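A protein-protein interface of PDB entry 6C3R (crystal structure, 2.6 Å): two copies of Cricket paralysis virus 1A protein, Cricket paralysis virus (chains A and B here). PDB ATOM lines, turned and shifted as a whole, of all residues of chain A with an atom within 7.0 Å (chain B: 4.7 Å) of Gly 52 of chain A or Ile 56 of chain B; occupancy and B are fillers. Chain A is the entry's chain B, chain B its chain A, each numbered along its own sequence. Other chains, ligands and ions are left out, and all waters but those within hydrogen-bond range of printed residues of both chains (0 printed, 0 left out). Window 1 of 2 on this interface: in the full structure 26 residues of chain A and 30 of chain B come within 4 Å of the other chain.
The guanidinium group (NH2) of Arg 55 of chain A sits close to the backbone NH (N) of Glu 94 of chain B (3.1 Å). SG of Cys 43 of chain A sits close to SG of Cys 53 of chain B (3.8 Å). The side-chain carboxylate (OE2) of Glu 94 of chain B lies close to the side-chain carboxylate (OD2) of Asp 50 of chain A (2.9 Å). The side-chain carboxylate (OE2) of Glu 94 of chain B lies close to the side-chain carboxylate (OD2) of Asp 54 of chain A (3.4 Å).
The side-chain carboxylate of Asp 50 of chain A sits at hydrogen-bond distance from the backbone NH of Gly 52 of chain A (3.3 Å). The side-chain hydroxyl (OG) of Ser 41 of chain B is in hydrogen-bond range of the side-chain carboxylate (OE2) of Glu 60 of chain B, at 2.9 Å. The side-chain sulfur (SG) of Cys 51 of chain A lies within hydrogen-bond range of the side-chain sulfur (SG) of Cys 53 of chain A, 3.6 Å away. The guanidinium group (NH1) of Arg 55 of chain B is in salt-bridge range of the side-chain carboxylate (OE1) of Glu 59 of chain B, at 2.6 Å. The backbone carbonyl oxygen of Ser 41 of chain B lies within hydrogen-bond range of the side-chain amino group of Lys 57 of chain B, 2.7 Å away. O of Cys 43 of chain A lies within hydrogen-bond range of SG of Cys 53 of chain A, at 3.5 Å.
Ser 41 of chain B touches Cys 51 of chain A. Cys 51 of chain A touches Ile 56 of chain B. O of Gly 52 of chain A touches CD1 of Ile 56 of chain B, at 3.7 Å. Ile 56 of chain A touches Gly 52 of chain B. CB of Asp 54 of chain B touches OE1 of Glu 94 of chain A (3.6 Å). Glu 94 of chain A touches Arg 55 of chain B (OE1 to N, 3.5 Å).
Of the printed residues of chain B, Gly 52 of chain A touches Ile 56. Printed residues of chain B within 4 Å of Ile 56 of chain A: Gly 52 (3.8 Å). Of the printed residues of chain B, Glu 94 of chain A touches Asp 54 and Arg 55. Of the printed residues of chain A, Ser 41 of chain B touches Cys 51. Of the printed residues of chain A, Asp 54 of chain B touches Glu 94 (3.6 Å). Printed residues of chain A within 4 Å of Arg 55 of chain B: Glu 94 (3.5 Å). Ile 56 of chain B touches just these residues of chain A: Cys 51 (3.6 Å) and Gly 52 (3.7 Å). Glu 60 of chain B touches none of the printed residues of chain A. The nearest residue of chain B that does not touch Gly 52 of chain A is Glu 94 of chain B (4.02 Å). The nearest residue of chain A that does not touch Ile 56 of chain B is Ile 56 of chain A (4.2 Å).
Printed residues of chain B that touch a printed residue of chain A: Ser 41, Gly 52, Cys 53, Asp 54, Arg 55, Ile 56 and Glu 94. Hydrophobic or aromatic side chains of chain A within 4 Å of the printed part of chain B: Ile 56. Among the printed residues, 10 pairs touch across the chains. Among the printed residues, no Asp or Glu carboxylate lies within 4 Å of a Lys or Arg side-chain nitrogen of the other chain.
Gly 52 of chain A touches Ile 56 of chain B, and with the chains exchanged Ile 56 of chain A touches Gly 52 of chain B. Asp 54 of chain A touches Glu 94 of chain B, and with the chains exchanged Glu 94 of chain A touches Asp 54 of chain B. Arg 55 of chain A touches Glu 94 of chain B, and with the chains exchanged Glu 94 of chain A touches Arg 55 of chain B. Positions printed for both chains: 52, 53, 54, 55, 56, 57 and 94.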
ATOM      1  N   CYS A  43      20.693   9.098  27.836  1.00  0.00           N
ATOM      2  CA  CYS A  43      21.241   8.155  26.863  1.00  0.00           C
ATOM      3  C   CYS A  43      22.606   8.444  26.260  1.00  0.00           C
ATOM      4  O   CYS A  43      23.020   9.596  26.117  1.00  0.00           O
ATOM      5  CB  CYS A  43      20.193   7.725  25.820  1.00  0.00           C
ATOM      6  SG  CYS A  43      19.633   8.574  24.317  1.00  0.00           S
ATOM      7  N   CYS A  45      25.891   6.692  23.540  1.00  0.00           N
ATOM      8  CA  CYS A  45      26.380   5.833  22.475  1.00  0.00           C
ATOM      9  C   CYS A  45      27.369   4.818  23.049  1.00  0.00           C
ATOM     10  O   CYS A  45      27.460   4.665  24.270  1.00  0.00           O
ATOM     11  CB  CYS A  45      27.051   6.699  21.402  1.00  0.00           C
ATOM     12  SG  CYS A  45      25.977   7.984  20.712  1.00  0.00           S
ATOM     13  N   PHE A  49      31.641   6.778  17.413  1.00  0.00           N
ATOM     14  CA  PHE A  49      30.377   6.833  16.625  1.00  0.00           C
ATOM     15  C   PHE A  49      29.224   7.661  17.204  1.00  0.00           C
ATOM     16  O   PHE A  49      28.723   7.378  18.298  1.00  0.00           O
ATOM     17  CB  PHE A  49      29.852   5.415  16.375  1.00  0.00           C
ATOM     18  CG  PHE A  49      28.683   5.359  15.437  1.00  0.00           C
ATOM     19  CD1 PHE A  49      28.841   5.675  14.103  1.00  0.00           C
ATOM     20  CD2 PHE A  49      27.425   4.997  15.893  1.00  0.00           C
ATOM     21  CE1 PHE A  49      27.759   5.636  13.239  1.00  0.00           C
ATOM     22  CE2 PHE A  49      26.342   4.952  15.042  1.00  0.00           C
ATOM     23  CZ  PHE A  49      26.503   5.273  13.711  1.00  0.00           C
ATOM     24  N   ASP A  50      28.805   8.670  16.446  1.00  0.00           N
ATOM     25  CA  ASP A  50      27.621   9.448  16.785  1.00  0.00           C
ATOM     26  C   ASP A  50      26.372   8.620  16.468  1.00  0.00           C
ATOM     27  O   ASP A  50      26.017   8.436  15.305  1.00  0.00           O
ATOM     28  CB  ASP A  50      27.601  10.781  16.024  1.00  0.00           C
ATOM     29  CG  ASP A  50      26.295  11.542  16.196  1.00  0.00           C
ATOM     30  OD1 ASP A  50      25.730  11.582  17.322  1.00  0.00           O
ATOM     31  OD2 ASP A  50      25.837  12.104  15.188  1.00  0.00           O
ATOM     32  N   CYS A  51      25.720   8.138  17.529  1.00  0.00           N
ATOM     33  CA  CYS A  51      24.500   7.341  17.449  1.00  0.00           C
ATOM     34  C   CYS A  51      23.192   8.150  17.485  1.00  0.00           C
ATOM     35  O   CYS A  51      22.120   7.563  17.460  1.00  0.00           O
ATOM     36  CB  CYS A  51      24.501   6.325  18.592  1.00  0.00           C
ATOM     37  SG  CYS A  51      24.226   7.015  20.242  1.00  0.00           S
ATOM     38  N   GLY A  52      23.263   9.476  17.558  1.00  0.00           N
ATOM     39  CA  GLY A  52      22.062  10.316  17.586  1.00  0.00           C
ATOM     40  C   GLY A  52      21.667  10.863  18.956  1.00  0.00           C
ATOM     41  O   GLY A  52      20.677  11.596  19.058  1.00  0.00           O
ATOM     42  N   CYS A  53      22.412  10.508  20.006  1.00  0.00           N
ATOM     43  CA  CYS A  53      22.201  11.092  21.329  1.00  0.00           C
ATOM     44  C   CYS A  53      22.473  12.600  21.382  1.00  0.00           C
ATOM     45  O   CYS A  53      21.747  13.328  22.065  1.00  0.00           O
ATOM     46  CB  CYS A  53      23.046  10.384  22.379  1.00  0.00           C
ATOM     47  SG  CYS A  53      22.413   8.753  22.802  1.00  0.00           S
ATOM     48  N   ASP A  54      23.501  13.047  20.660  1.00  0.00           N
ATOM     49  CA  ASP A  54      23.878  14.457  20.595  1.00  0.00           C
ATOM     50  C   ASP A  54      22.721  15.358  20.209  1.00  0.00           C
ATOM     51  O   ASP A  54      22.553  16.422  20.786  1.00  0.00           O
ATOM     52  CB  ASP A  54      25.010  14.662  19.575  1.00  0.00           C
ATOM     53  CG  ASP A  54      26.324  14.022  20.011  1.00  0.00           C
ATOM     54  OD1 ASP A  54      26.402  13.513  21.162  1.00  0.00           O
ATOM     55  OD2 ASP A  54      27.287  14.025  19.205  1.00  0.00           O
ATOM     56  N   ARG A  55      21.934  14.935  19.223  1.00  0.00           N
ATOM     57  CA  ARG A  55      20.786  15.716  18.799  1.00  0.00           C
ATOM     58  C   ARG A  55      19.726  15.846  19.906  1.00  0.00           C
ATOM     59  O   ARG A  55      19.098  16.883  20.016  1.00  0.00           O
ATOM     60  CB  ARG A  55      20.172  15.143  17.511  1.00  0.00           C
ATOM     61  CG  ARG A  55      18.926  15.894  17.040  1.00  0.00           C
ATOM     62  CD  ARG A  55      18.155  15.170  15.955  1.00  0.00           C
ATOM     63  NE  ARG A  55      18.956  15.048  14.741  1.00  0.00           N
ATOM     64  CZ  ARG A  55      19.246  16.040  13.891  1.00  0.00           C
ATOM     65  NH1 ARG A  55      18.805  17.283  14.066  1.00  0.00           N
ATOM     66  NH2 ARG A  55      19.972  15.773  12.830  1.00  0.00           N
ATOM     67  N   ILE A  56      19.528  14.810  20.710  1.00  0.00           N
ATOM     68  CA  ILE A  56      18.531  14.849  21.795  1.00  0.00           C
ATOM     69  C   ILE A  56      18.971  15.758  22.939  1.00  0.00           C
ATOM     70  O   ILE A  56      18.194  16.559  23.439  1.00  0.00           O
ATOM     71  CB  ILE A  56      18.255  13.438  22.375  1.00  0.00           C
ATOM     72  CG1 ILE A  56      17.546  12.554  21.342  1.00  0.00           C
ATOM     73  CG2 ILE A  56      17.399  13.527  23.640  1.00  0.00           C
ATOM     74  CD1 ILE A  56      17.583  11.073  21.683  1.00  0.00           C
ATOM     75  N   LYS A  57      20.216  15.586  23.362  1.00  0.00           N
ATOM     76  CA  LYS A  57      20.813  16.424  24.389  1.00  0.00           C
ATOM     77  C   LYS A  57      20.744  17.903  24.009  1.00  0.00           C
ATOM     78  O   LYS A  57      20.393  18.740  24.837  1.00  0.00           O
ATOM     79  CB  LYS A  57      22.261  15.995  24.672  1.00  0.00           C
ATOM     80  CG  LYS A  57      22.434  14.598  25.282  1.00  0.00           C
ATOM     81  CD  LYS A  57      21.604  14.372  26.543  1.00  0.00           C
ATOM     82  CE  LYS A  57      21.975  13.073  27.243  1.00  0.00           C
ATOM     83  NZ  LYS A  57      21.302  12.906  28.575  1.00  0.00           N
ATOM     84  N   GLU A  94       9.478  11.951  13.562  1.00  0.00           N
ATOM     85  CA  GLU A  94       9.691  10.516  13.297  1.00  0.00           C
ATOM     86  C   GLU A  94       8.692  10.064  12.226  1.00  0.00           C
ATOM     87  O   GLU A  94       7.481  10.203  12.422  1.00  0.00           O
ATOM     88  CB  GLU A  94       9.526   9.683  14.580  1.00  0.00           C
ATOM     89  CG  GLU A  94       9.910   8.209  14.429  1.00  0.00           C
ATOM     90  CD  GLU A  94      10.048   7.453  15.747  1.00  0.00           C
ATOM     91  OE1 GLU A  94       9.952   8.067  16.835  1.00  0.00           O
ATOM     92  OE2 GLU A  94      10.262   6.223  15.692  1.00  0.00           O
ATOM     93  N   SER B  41      23.000   2.325  20.904  1.00  0.00           N
ATOM     94  CA  SER B  41      22.909   3.221  22.054  1.00  0.00           C
ATOM     95  C   SER B  41      22.113   2.533  23.133  1.00  0.00           C
ATOM     96  O   SER B  41      21.469   1.519  22.871  1.00  0.00           O
ATOM     97  CB  SER B  41      22.160   4.497  21.660  1.00  0.00           C
ATOM     98  OG  SER B  41      20.770   4.247  21.487  1.00  0.00           O
ATOM     99  N   GLY B  52      12.747  10.996  21.657  1.00  0.00           N
ATOM    100  CA  GLY B  52      13.470  10.685  20.425  1.00  0.00           C
ATOM    101  C   GLY B  52      14.334   9.445  20.462  1.00  0.00           C
ATOM    102  O   GLY B  52      15.027   9.169  19.490  1.00  0.00           O
ATOM    103  N   CYS B  53      14.310   8.706  21.571  1.00  0.00           N
ATOM    104  CA  CYS B  53      15.015   7.436  21.665  1.00  0.00           C
ATOM    105  C   CYS B  53      14.452   6.402  20.706  1.00  0.00           C
ATOM    106  O   CYS B  53      15.207   5.571  20.206  1.00  0.00           O
ATOM    107  CB  CYS B  53      14.968   6.865  23.086  1.00  0.00           C
ATOM    108  SG  CYS B  53      15.927   7.780  24.320  1.00  0.00           S
ATOM    109  N   ASP B  54      13.135   6.443  20.478  1.00  0.00           N
ATOM    110  CA  ASP B  54      12.473   5.547  19.542  1.00  0.00           C
ATOM    111  C   ASP B  54      13.051   5.694  18.148  1.00  0.00           C
ATOM    112  O   ASP B  54      13.364   4.708  17.495  1.00  0.00           O
ATOM    113  CB  ASP B  54      10.980   5.847  19.456  1.00  0.00           C
ATOM    114  CG  ASP B  54      10.211   5.519  20.745  1.00  0.00           C
ATOM    115  OD1 ASP B  54      10.641   4.685  21.580  1.00  0.00           O
ATOM    116  OD2 ASP B  54       9.132   6.122  20.906  1.00  0.00           O
ATOM    117  N   ARG B  55      13.159   6.938  17.698  1.00  0.00           N
ATOM    118  CA  ARG B  55      13.762   7.271  16.397  1.00  0.00           C
ATOM    119  C   ARG B  55      15.136   6.590  16.283  1.00  0.00           C
ATOM    120  O   ARG B  55      15.414   5.914  15.320  1.00  0.00           O
ATOM    121  CB  ARG B  55      13.865   8.797  16.262  1.00  0.00           C
ATOM    122  CG  ARG B  55      13.609   9.402  14.886  1.00  0.00           C
ATOM    123  CD  ARG B  55      14.869   9.562  14.059  1.00  0.00           C
ATOM    124  NE  ARG B  55      15.988  10.122  14.833  1.00  0.00           N
ATOM    125  CZ  ARG B  55      17.284   9.988  14.525  1.00  0.00           C
ATOM    126  NH1 ARG B  55      17.691   9.339  13.418  1.00  0.00           N
ATOM    127  NH2 ARG B  55      18.198  10.531  15.335  1.00  0.00           N
ATOM    128  N   ILE B  56      15.953   6.733  17.323  1.00  0.00           N
ATOM    129  CA  ILE B  56      17.264   6.065  17.444  1.00  0.00           C
ATOM    130  C   ILE B  56      17.105   4.546  17.315  1.00  0.00           C
ATOM    131  O   ILE B  56      17.776   3.919  16.509  1.00  0.00           O
ATOM    132  CB  ILE B  56      17.970   6.369  18.817  1.00  0.00           C
ATOM    133  CG1 ILE B  56      18.161   7.862  19.091  1.00  0.00           C
ATOM    134  CG2 ILE B  56      19.310   5.684  18.919  1.00  0.00           C
ATOM    135  CD1 ILE B  56      18.740   8.635  17.935  1.00  0.00           C
ATOM    136  N   LYS B  57      16.238   3.963  18.130  1.00  0.00           N
ATOM    137  CA  LYS B  57      16.104   2.506  18.196  1.00  0.00           C
ATOM    138  C   LYS B  57      15.632   1.884  16.877  1.00  0.00           C
ATOM    139  O   LYS B  57      16.176   0.879  16.420  1.00  0.00           O
ATOM    140  CB  LYS B  57      15.181   2.117  19.346  1.00  0.00           C
ATOM    141  CG  LYS B  57      15.811   2.354  20.713  1.00  0.00           C
ATOM    142  CD  LYS B  57      16.808   1.251  21.045  1.00  0.00           C
ATOM    143  CE  LYS B  57      18.033   1.770  21.789  1.00  0.00           C
ATOM    144  NZ  LYS B  57      19.111   0.736  21.814  1.00  0.00           N
ATOM    145  N   ARG B  58      14.644   2.520  16.269  1.00  0.00           N
ATOM    146  CA  ARG B  58      14.227   2.221  14.903  1.00  0.00           C
ATOM    147  C   ARG B  58      15.374   2.246  13.867  1.00  0.00           C
ATOM    148  O   ARG B  58      15.447   1.355  13.022  1.00  0.00           O
ATOM    149  CB  ARG B  58      13.113   3.183  14.498  1.00  0.00           C
ATOM    150  CG  ARG B  58      12.608   3.038  13.080  1.00  0.00           C
ATOM    151  CD  ARG B  58      11.867   1.729  12.860  1.00  0.00           C
ATOM    152  NE  ARG B  58      11.004   1.839  11.676  1.00  0.00           N
ATOM    153  CZ  ARG B  58      10.520   0.823  10.964  1.00  0.00           C
ATOM    154  NH1 ARG B  58      10.772  -0.447  11.295  1.00  0.00           N
ATOM    155  NH2 ARG B  58       9.759   1.082   9.906  1.00  0.00           N
ATOM    156  N   GLU B  59      16.238   3.255  13.931  1.00  0.00           N
ATOM    157  CA  GLU B  59      17.391   3.361  13.027  1.00  0.00           C
ATOM    158  C   GLU B  59      18.344   2.150  13.169  1.00  0.00           C
ATOM    159  O   GLU B  59      18.753   1.540  12.180  1.00  0.00           O
ATOM    160  CB  GLU B  59      18.128   4.707  13.225  1.00  0.00           C
ATOM    161  CG  GLU B  59      19.172   5.009  12.134  1.00  0.00           C
ATOM    162  CD  GLU B  59      19.646   6.477  12.042  1.00  0.00           C
ATOM    163  OE1 GLU B  59      18.819   7.411  12.007  1.00  0.00           O
ATOM    164  OE2 GLU B  59      20.869   6.720  11.966  1.00  0.00           O
ATOM    165  N   GLU B  60      18.652   1.777  14.410  1.00  0.00           N
ATOM    166  CA  GLU B  60      19.511   0.609  14.709  1.00  0.00           C
ATOM    167  C   GLU B  60      18.905  -0.709  14.216  1.00  0.00           C
ATOM    168  O   GLU B  60      19.602  -1.570  13.719  1.00  0.00           O
ATOM    169  CB  GLU B  60      19.747   0.496  16.219  1.00  0.00           C
ATOM    170  CG  GLU B  60      20.478   1.676  16.849  1.00  0.00           C
ATOM    171  CD  GLU B  60      20.382   1.724  18.386  1.00  0.00           C
ATOM    172  OE1 GLU B  60      19.951   0.708  19.027  1.00  0.00           O
ATOM    173  OE2 GLU B  60      20.762   2.793  18.953  1.00  0.00           O
ATOM    174  N   GLU B  94      22.442  14.884  11.203  1.00  0.00           N
ATOM    175  CA  GLU B  94      23.019  15.630  12.359  1.00  0.00           C
ATOM    176  C   GLU B  94      23.876  16.786  11.867  1.00  0.00           C
ATOM    177  O   GLU B  94      25.110  16.720  11.837  1.00  0.00           O
ATOM    178  CB  GLU B  94      23.785  14.729  13.357  1.00  0.00           C
ATOM    179  CG  GLU B  94      24.195  15.472  14.636  1.00  0.00           C
ATOM    180  CD  GLU B  94      24.550  14.563  15.808  1.00  0.00           C
ATOM    181  OE1 GLU B  94      23.716  13.718  16.216  1.00  0.00           O
ATOM    182  OE2 GLU B  94      25.670  14.710  16.340  1.00  0.00           O
